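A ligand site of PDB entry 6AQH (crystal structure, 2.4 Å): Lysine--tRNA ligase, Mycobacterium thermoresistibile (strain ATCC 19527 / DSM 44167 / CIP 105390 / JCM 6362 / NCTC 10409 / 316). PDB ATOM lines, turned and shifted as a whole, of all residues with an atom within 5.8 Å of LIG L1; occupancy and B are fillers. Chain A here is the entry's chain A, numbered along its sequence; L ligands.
Residues that only touch LIG L1: Arg 266 (3.4 Å), Glu 268 (3.99 Å), Thr 273 (3.7 Å), His 274 (3.6 Å), Phe 278 (3.4 Å), Met 280 (3.9 Å), Glu 427 (3.6 Å), Leu 428 (3.7 Å), Ala 429 (3.8 Å), Thr 430 (3.7 Å), Gly 481 (3.2 Å), Met 482 (3.9 Å) and Ile 496 (3.97 Å). Hydrophobic or aromatic side chains that line LIG L1: His 274, Phe 278, Met 280 and Ile 496.
A ring nitrogen (NE2) of His 274 lies close to the guanidinium group of Arg 486 (3.4 Å). The backbone carbonyl oxygen (O) of Glu 427 lies within hydrogen-bond range of the guanidinium group (NH1) of Arg 486, at 3.0 Å. NH2 of Arg 486 is in hydrogen-bond range of O of Thr 273. O of Gly 481 lies within hydrogen-bond range of N of Thr 430 (2.8 Å). O of Pro 276 is in hydrogen-bond range of N of Arg 266 (2.9 Å). A ring nitrogen (ND1) of His 274 is in hydrogen-bond range of the side-chain hydroxyl (OG1) of Thr 273 (2.8 Å). The side-chain hydroxyl of Thr 430 lies close to the side-chain carboxylate of Asp 420, at 3.4 Å. SD of Met 280 is in hydrogen-bond range of N of Glu 282 (3.7 Å).
The backbone NH (N) of Ser 275 is in hydrogen-bond range of an oxygen (O3) of LIG L1 (3.0 Å). The backbone carbonyl oxygen (O) of Ser 275 sits close to an oxygen (O3) of LIG L1, at 3.5 Å. The guanidinium group (NE) of Arg 486 lies within hydrogen-bond range of an oxygen (O1) of LIG L1. N of Gly 483 is in hydrogen-bond range of O5 of LIG L1, 3.3 Å away. NH2 of Arg 266 lies within salt-bridge range of O1 of LG2 L2. The side-chain carboxylate (OE1) of Glu 282 lies within salt-bridge range of a nitrogen (N1) of LG2 L2 (2.9 Å).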
ATOM      1  N   ALA A 223      -7.887   4.046   4.238  1.00  0.00           N
ATOM      2  CA  ALA A 223      -8.724   3.005   3.639  1.00  0.00           C
ATOM      3  C   ALA A 223      -8.153   2.641   2.276  1.00  0.00           C
ATOM      4  O   ALA A 223      -7.374   3.396   1.687  1.00  0.00           O
ATOM      5  CB  ALA A 223     -10.182   3.454   3.506  1.00  0.00           C
ATOM      6  N   ARG A 266     -14.755   3.329   0.019  1.00  0.00           N
ATOM      7  CA  ARG A 266     -13.661   2.675   0.709  1.00  0.00           C
ATOM      8  C   ARG A 266     -13.786   1.171   0.466  1.00  0.00           C
ATOM      9  O   ARG A 266     -14.705   0.534   0.974  1.00  0.00           O
ATOM     10  CB  ARG A 266     -13.668   3.007   2.198  1.00  0.00           C
ATOM     11  CG  ARG A 266     -13.633   4.500   2.460  1.00  0.00           C
ATOM     12  CD  ARG A 266     -13.552   4.839   3.946  1.00  0.00           C
ATOM     13  NE  ARG A 266     -13.618   6.279   4.153  1.00  0.00           N
ATOM     14  CZ  ARG A 266     -13.458   6.882   5.330  1.00  0.00           C
ATOM     15  NH1 ARG A 266     -13.207   6.170   6.420  1.00  0.00           N
ATOM     16  NH2 ARG A 266     -13.537   8.204   5.418  1.00  0.00           N
ATOM     17  N   ASN A 267     -12.852   0.619  -0.314  1.00  0.00           N
ATOM     18  CA  ASN A 267     -12.949  -0.755  -0.816  1.00  0.00           C
ATOM     19  C   ASN A 267     -12.421  -1.735   0.232  1.00  0.00           C
ATOM     20  O   ASN A 267     -11.356  -2.341   0.083  1.00  0.00           O
ATOM     21  CB  ASN A 267     -12.211  -0.876  -2.135  1.00  0.00           C
ATOM     22  CG  ASN A 267     -12.453  -2.201  -2.824  1.00  0.00           C
ATOM     23  OD1 ASN A 267     -13.423  -2.900  -2.527  1.00  0.00           O
ATOM     24  ND2 ASN A 267     -11.569  -2.561  -3.747  1.00  0.00           N
ATOM     25  N   GLU A 268     -13.201  -1.898   1.297  1.00  0.00           N
ATOM     26  CA  GLU A 268     -12.842  -2.812   2.382  1.00  0.00           C
ATOM     27  C   GLU A 268     -14.058  -3.684   2.686  1.00  0.00           C
ATOM     28  O   GLU A 268     -15.000  -3.797   1.901  1.00  0.00           O
ATOM     29  CB  GLU A 268     -12.344  -2.019   3.599  1.00  0.00           C
ATOM     30  CG  GLU A 268     -11.053  -1.249   3.348  1.00  0.00           C
ATOM     31  CD  GLU A 268     -10.601  -0.450   4.559  1.00  0.00           C
ATOM     32  OE1 GLU A 268      -9.398  -0.464   4.865  1.00  0.00           O
ATOM     33  OE2 GLU A 268     -11.465   0.175   5.203  1.00  0.00           O
ATOM     34  N   GLY A 269     -14.049  -4.311   3.865  1.00  0.00           N
ATOM     35  CA  GLY A 269     -15.099  -5.242   4.223  1.00  0.00           C
ATOM     36  C   GLY A 269     -16.379  -4.546   4.628  1.00  0.00           C
ATOM     37  O   GLY A 269     -16.379  -3.456   5.190  1.00  0.00           O
ATOM     38  N   THR A 273     -21.652  -2.125  10.419  1.00  0.00           N
ATOM     39  CA  THR A 273     -21.317  -0.720  10.564  1.00  0.00           C
ATOM     40  C   THR A 273     -20.506  -0.171   9.391  1.00  0.00           C
ATOM     41  O   THR A 273     -20.206   1.028   9.384  1.00  0.00           O
ATOM     42  CB  THR A 273     -20.526  -0.486  11.863  1.00  0.00           C
ATOM     43  OG1 THR A 273     -19.274  -1.181  11.802  1.00  0.00           O
ATOM     44  CG2 THR A 273     -21.317  -0.983  13.067  1.00  0.00           C
ATOM     45  N   HIS A 274     -20.162  -0.995   8.411  1.00  0.00           N
ATOM     46  CA  HIS A 274     -19.354  -0.558   7.276  1.00  0.00           C
ATOM     47  C   HIS A 274     -20.046  -0.915   5.978  1.00  0.00           C
ATOM     48  O   HIS A 274     -20.521  -2.048   5.808  1.00  0.00           O
ATOM     49  CB  HIS A 274     -17.949  -1.182   7.306  1.00  0.00           C
ATOM     50  CG  HIS A 274     -17.112  -0.719   8.453  1.00  0.00           C
ATOM     51  ND1 HIS A 274     -17.340  -1.109   9.752  1.00  0.00           N
ATOM     52  CD2 HIS A 274     -16.025   0.090   8.488  1.00  0.00           C
ATOM     53  CE1 HIS A 274     -16.444  -0.548  10.543  1.00  0.00           C
ATOM     54  NE2 HIS A 274     -15.627   0.190   9.796  1.00  0.00           N
ATOM     55  N   SER A 275     -20.111   0.053   5.060  1.00  0.00           N
ATOM     56  CA  SER A 275     -20.585  -0.165   3.704  1.00  0.00           C
ATOM     57  C   SER A 275     -19.560   0.441   2.756  1.00  0.00           C
ATOM     58  O   SER A 275     -19.211   1.624   2.918  1.00  0.00           O
ATOM     59  CB  SER A 275     -21.968   0.462   3.491  1.00  0.00           C
ATOM     60  OG  SER A 275     -22.383   0.336   2.135  1.00  0.00           O
ATOM     61  N   PRO A 276     -19.053  -0.322   1.782  1.00  0.00           N
ATOM     62  CA  PRO A 276     -17.997   0.218   0.901  1.00  0.00           C
ATOM     63  C   PRO A 276     -18.383   1.533   0.234  1.00  0.00           C
ATOM     64  O   PRO A 276     -17.535   2.434   0.116  1.00  0.00           O
ATOM     65  CB  PRO A 276     -17.807  -0.904  -0.130  1.00  0.00           C
ATOM     66  CG  PRO A 276     -18.234  -2.139   0.592  1.00  0.00           C
ATOM     67  CD  PRO A 276     -19.375  -1.714   1.468  1.00  0.00           C
ATOM     68  N   PHE A 278     -20.750   4.701   0.909  1.00  0.00           N
ATOM     69  CA  PHE A 278     -21.520   5.303   1.983  1.00  0.00           C
ATOM     70  C   PHE A 278     -21.406   6.823   1.885  1.00  0.00           C
ATOM     71  O   PHE A 278     -20.583   7.358   1.136  1.00  0.00           O
ATOM     72  CB  PHE A 278     -21.055   4.802   3.354  1.00  0.00           C
ATOM     73  CG  PHE A 278     -19.686   5.266   3.755  1.00  0.00           C
ATOM     74  CD1 PHE A 278     -18.553   4.670   3.223  1.00  0.00           C
ATOM     75  CD2 PHE A 278     -19.521   6.281   4.676  1.00  0.00           C
ATOM     76  CE1 PHE A 278     -17.279   5.091   3.594  1.00  0.00           C
ATOM     77  CE2 PHE A 278     -18.264   6.713   5.055  1.00  0.00           C
ATOM     78  CZ  PHE A 278     -17.134   6.113   4.511  1.00  0.00           C
ATOM     79  N   MET A 280     -20.938  10.593   3.694  1.00  0.00           N
ATOM     80  CA  MET A 280     -20.251  11.262   4.788  1.00  0.00           C
ATOM     81  C   MET A 280     -20.625  12.743   4.792  1.00  0.00           C
ATOM     82  O   MET A 280     -21.196  13.280   3.844  1.00  0.00           O
ATOM     83  CB  MET A 280     -18.735  11.103   4.677  1.00  0.00           C
ATOM     84  CG  MET A 280     -18.131  11.669   3.398  1.00  0.00           C
ATOM     85  SD  MET A 280     -17.801  13.450   3.432  1.00  0.00           S
ATOM     86  CE  MET A 280     -18.299  13.909   1.777  1.00  0.00           C
ATOM     87  N   LEU A 281     -20.275  13.415   5.888  1.00  0.00           N
ATOM     88  CA  LEU A 281     -20.355  14.864   5.995  1.00  0.00           C
ATOM     89  C   LEU A 281     -19.009  15.378   6.486  1.00  0.00           C
ATOM     90  O   LEU A 281     -18.521  14.944   7.528  1.00  0.00           O
ATOM     91  CB  LEU A 281     -21.470  15.292   6.956  1.00  0.00           C
ATOM     92  CG  LEU A 281     -21.450  16.784   7.307  1.00  0.00           C
ATOM     93  CD1 LEU A 281     -21.756  17.640   6.090  1.00  0.00           C
ATOM     94  CD2 LEU A 281     -22.407  17.094   8.444  1.00  0.00           C
ATOM     95  N   GLU A 282     -18.412  16.300   5.726  1.00  0.00           N
ATOM     96  CA  GLU A 282     -17.169  16.932   6.119  1.00  0.00           C
ATOM     97  C   GLU A 282     -17.359  18.445   6.080  1.00  0.00           C
ATOM     98  O   GLU A 282     -17.707  18.993   5.031  1.00  0.00           O
ATOM     99  CB  GLU A 282     -16.011  16.518   5.204  1.00  0.00           C
ATOM    100  CG  GLU A 282     -15.257  15.291   5.684  1.00  0.00           C
ATOM    101  CD  GLU A 282     -13.900  15.143   5.026  1.00  0.00           C
ATOM    102  OE1 GLU A 282     -13.401  14.000   4.899  1.00  0.00           O
ATOM    103  OE2 GLU A 282     -13.322  16.178   4.633  1.00  0.00           O
ATOM    104  N   ASP A 420     -13.075  12.435  19.029  1.00  0.00           N
ATOM    105  CA  ASP A 420     -13.877  11.364  18.447  1.00  0.00           C
ATOM    106  C   ASP A 420     -15.193  11.280  19.203  1.00  0.00           C
ATOM    107  O   ASP A 420     -15.198  11.259  20.433  1.00  0.00           O
ATOM    108  CB  ASP A 420     -13.138  10.026  18.507  1.00  0.00           C
ATOM    109  CG  ASP A 420     -12.864   9.453  17.130  1.00  0.00           C
ATOM    110  OD1 ASP A 420     -13.287  10.066  16.126  1.00  0.00           O
ATOM    111  OD2 ASP A 420     -12.220   8.375  17.050  1.00  0.00           O
ATOM    112  N   GLU A 427     -18.439   4.915  16.381  1.00  0.00           N
ATOM    113  CA  GLU A 427     -17.797   6.178  16.033  1.00  0.00           C
ATOM    114  C   GLU A 427     -18.685   6.945  15.059  1.00  0.00           C
ATOM    115  O   GLU A 427     -18.804   6.577  13.892  1.00  0.00           O
ATOM    116  CB  GLU A 427     -16.415   5.938  15.431  1.00  0.00           C
ATOM    117  CG  GLU A 427     -15.766   7.205  14.887  1.00  0.00           C
ATOM    118  CD  GLU A 427     -14.463   6.926  14.150  1.00  0.00           C
ATOM    119  OE1 GLU A 427     -13.440   7.552  14.502  1.00  0.00           O
ATOM    120  OE2 GLU A 427     -14.473   6.091  13.228  1.00  0.00           O
ATOM    121  N   LEU A 428     -19.317   8.013  15.547  1.00  0.00           N
ATOM    122  CA  LEU A 428     -20.240   8.788  14.741  1.00  0.00           C
ATOM    123  C   LEU A 428     -19.536   9.931  14.001  1.00  0.00           C
ATOM    124  O   LEU A 428     -19.747  10.105  12.798  1.00  0.00           O
ATOM    125  CB  LEU A 428     -21.365   9.346  15.614  1.00  0.00           C
ATOM    126  CG  LEU A 428     -22.373  10.292  14.949  1.00  0.00           C
ATOM    127  CD1 LEU A 428     -22.971   9.659  13.704  1.00  0.00           C
ATOM    128  CD2 LEU A 428     -23.454  10.672  15.940  1.00  0.00           C
ATOM    129  N   ALA A 429     -18.717  10.697  14.705  1.00  0.00           N
ATOM    130  CA  ALA A 429     -18.084  11.861  14.100  1.00  0.00           C
ATOM    131  C   ALA A 429     -16.677  12.041  14.665  1.00  0.00           C
ATOM    132  O   ALA A 429     -16.325  11.487  15.706  1.00  0.00           O
ATOM    133  CB  ALA A 429     -18.908  13.126  14.318  1.00  0.00           C
ATOM    134  N   THR A 430     -15.889  12.842  13.950  1.00  0.00           N
ATOM    135  CA  THR A 430     -14.539  13.196  14.378  1.00  0.00           C
ATOM    136  C   THR A 430     -14.280  14.648  14.004  1.00  0.00           C
ATOM    137  O   THR A 430     -14.977  15.230  13.166  1.00  0.00           O
ATOM    138  CB  THR A 430     -13.479  12.286  13.733  1.00  0.00           C
ATOM    139  OG1 THR A 430     -12.181  12.649  14.233  1.00  0.00           O
ATOM    140  CG2 THR A 430     -13.495  12.439  12.225  1.00  0.00           C
ATOM    141  N   GLY A 481     -15.759  15.326  10.385  1.00  0.00           N
ATOM    142  CA  GLY A 481     -16.197  14.255   9.524  1.00  0.00           C
ATOM    143  C   GLY A 481     -17.265  13.429  10.227  1.00  0.00           C
ATOM    144  O   GLY A 481     -17.147  13.190  11.431  1.00  0.00           O
ATOM    145  N   MET A 482     -18.294  13.002   9.502  1.00  0.00           N
ATOM    146  CA  MET A 482     -19.376  12.248  10.116  1.00  0.00           C
ATOM    147  C   MET A 482     -20.029  11.355   9.081  1.00  0.00           C
ATOM    148  O   MET A 482     -20.390  11.819   7.988  1.00  0.00           O
ATOM    149  CB  MET A 482     -20.420  13.178  10.742  1.00  0.00           C
ATOM    150  CG  MET A 482     -21.571  12.446  11.420  1.00  0.00           C
ATOM    151  SD  MET A 482     -22.736  13.544  12.252  1.00  0.00           S
ATOM    152  CE  MET A 482     -23.426  14.423  10.851  1.00  0.00           C
ATOM    153  N   GLY A 483     -20.183  10.079   9.422  1.00  0.00           N
ATOM    154  CA  GLY A 483     -20.892   9.148   8.561  1.00  0.00           C
ATOM    155  C   GLY A 483     -22.396   9.293   8.704  1.00  0.00           C
ATOM    156  O   GLY A 483     -22.958   8.996   9.758  1.00  0.00           O
ATOM    157  N   ASP A 485     -24.760   7.608   7.283  1.00  0.00           N
ATOM    158  CA  ASP A 485     -25.396   6.309   7.481  1.00  0.00           C
ATOM    159  C   ASP A 485     -25.361   5.892   8.943  1.00  0.00           C
ATOM    160  O   ASP A 485     -26.316   5.309   9.458  1.00  0.00           O
ATOM    161  CB  ASP A 485     -24.713   5.267   6.602  1.00  0.00           C
ATOM    162  CG  ASP A 485     -24.468   5.764   5.194  1.00  0.00           C
ATOM    163  OD1 ASP A 485     -25.416   5.745   4.378  1.00  0.00           O
ATOM    164  OD2 ASP A 485     -23.335   6.210   4.909  1.00  0.00           O
ATOM    165  N   ARG A 486     -24.257   6.201   9.635  1.00  0.00           N
ATOM    166  CA  ARG A 486     -24.186   5.932  11.068  1.00  0.00           C
ATOM    167  C   ARG A 486     -25.018   6.927  11.856  1.00  0.00           C
ATOM    168  O   ARG A 486     -25.482   6.610  12.960  1.00  0.00           O
ATOM    169  CB  ARG A 486     -22.732   5.951  11.529  1.00  0.00           C
ATOM    170  CG  ARG A 486     -21.897   4.817  10.957  1.00  0.00           C
ATOM    171  CD  ARG A 486     -20.498   4.791  11.554  1.00  0.00           C
ATOM    172  NE  ARG A 486     -19.770   3.593  11.155  1.00  0.00           N
ATOM    173  CZ  ARG A 486     -18.547   3.282  11.579  1.00  0.00           C
ATOM    174  NH1 ARG A 486     -17.915   4.087  12.427  1.00  0.00           N
ATOM    175  NH2 ARG A 486     -17.968   2.173  11.158  1.00  0.00           N
ATOM    176  N   ILE A 496     -27.249  -0.680   9.051  1.00  0.00           N
ATOM    177  CA  ILE A 496     -26.686   0.236   8.064  1.00  0.00           C
ATOM    178  C   ILE A 496     -27.276  -0.023   6.691  1.00  0.00           C
ATOM    179  O   ILE A 496     -27.412   0.921   5.884  1.00  0.00           O
ATOM    180  CB  ILE A 496     -25.151   0.126   8.055  1.00  0.00           C
ATOM    181  CG1 ILE A 496     -24.533   1.218   7.171  1.00  0.00           C
ATOM    182  CG2 ILE A 496     -24.699  -1.257   7.583  1.00  0.00           C
ATOM    183  CD1 ILE A 496     -23.027   1.192   7.111  1.00  0.00           C
HETATM  184  O1  LIG L   1     -19.792   4.478   8.155  1.00  0.00           O
HETATM  185  C1  LIG L   1     -18.600   4.522   8.160  1.00  0.00           C
HETATM  186  C2  LIG L   1     -17.690   3.741   7.295  1.00  0.00           C
HETATM  187  C3  LIG L   1     -16.312   3.830   7.444  1.00  0.00           C
HETATM  188  C4  LIG L   1     -15.460   3.098   6.632  1.00  0.00           C
HETATM  189  C5  LIG L   1     -15.980   2.273   5.662  1.00  0.00           C
HETATM  190  O2  LIG L   1     -15.203   1.518   4.831  1.00  0.00           O
HETATM  191  C6  LIG L   1     -17.348   2.174   5.499  1.00  0.00           C
HETATM  192  C7  LIG L   1     -18.204   2.901   6.298  1.00  0.00           C
HETATM  193  O3  LIG L   1     -19.540   2.817   6.144  1.00  0.00           O
HETATM  194  O4  LIG L   1     -17.998   5.390   9.040  1.00  0.00           O
HETATM  195  C8  LIG L   1     -16.655   5.893   8.850  1.00  0.00           C
HETATM  196  C9  LIG L   1     -15.723   4.731   8.516  1.00  0.00           C
HETATM  197  C10 LIG L   1     -16.165   6.687  10.061  1.00  0.00           C
HETATM  198  C11 LIG L   1     -17.070   7.857  10.462  1.00  0.00           C
HETATM  199  O5  LIG L   1     -17.164   8.661   9.254  1.00  0.00           O
HETATM  200  C12 LIG L   1     -15.978   9.366   8.813  1.00  0.00           C
HETATM  201  C13 LIG L   1     -16.265  10.214   7.571  1.00  0.00           C
HETATM  202  C14 LIG L   1     -15.369  10.190   9.968  1.00  0.00           C
HETATM  203  C15 LIG L   1     -16.273  10.145  11.203  1.00  0.00           C
HETATM  204  C16 LIG L   1     -16.520   8.688  11.629  1.00  0.00           C
HETATM  205  N1  LG2 L   2     -11.175  12.849   6.453  1.00  0.00           N
HETATM  206  C1  LG2 L   2     -11.715  12.419   7.731  1.00  0.00           C
HETATM  207  C2  LG2 L   2     -12.166  10.957   7.636  1.00  0.00           C
HETATM  208  O1  LG2 L   2     -12.458  10.462   6.519  1.00  0.00           O
HETATM  209  C3  LG2 L   2     -12.885  13.310   8.150  1.00  0.00           C
HETATM  210  C4  LG2 L   2     -12.394  14.748   8.358  1.00  0.00           C
HETATM  211  C5  LG2 L   2     -11.648  14.848   9.683  1.00  0.00           C
HETATM  212  C6  LG2 L   2     -11.422  16.311  10.037  1.00  0.00           C
HETATM  213  N2  LG2 L   2     -10.437  16.886   9.140  1.00  0.00           N
HETATM  214  O2  LG2 L   2     -12.251  10.261   8.678  1.00  0.00           O
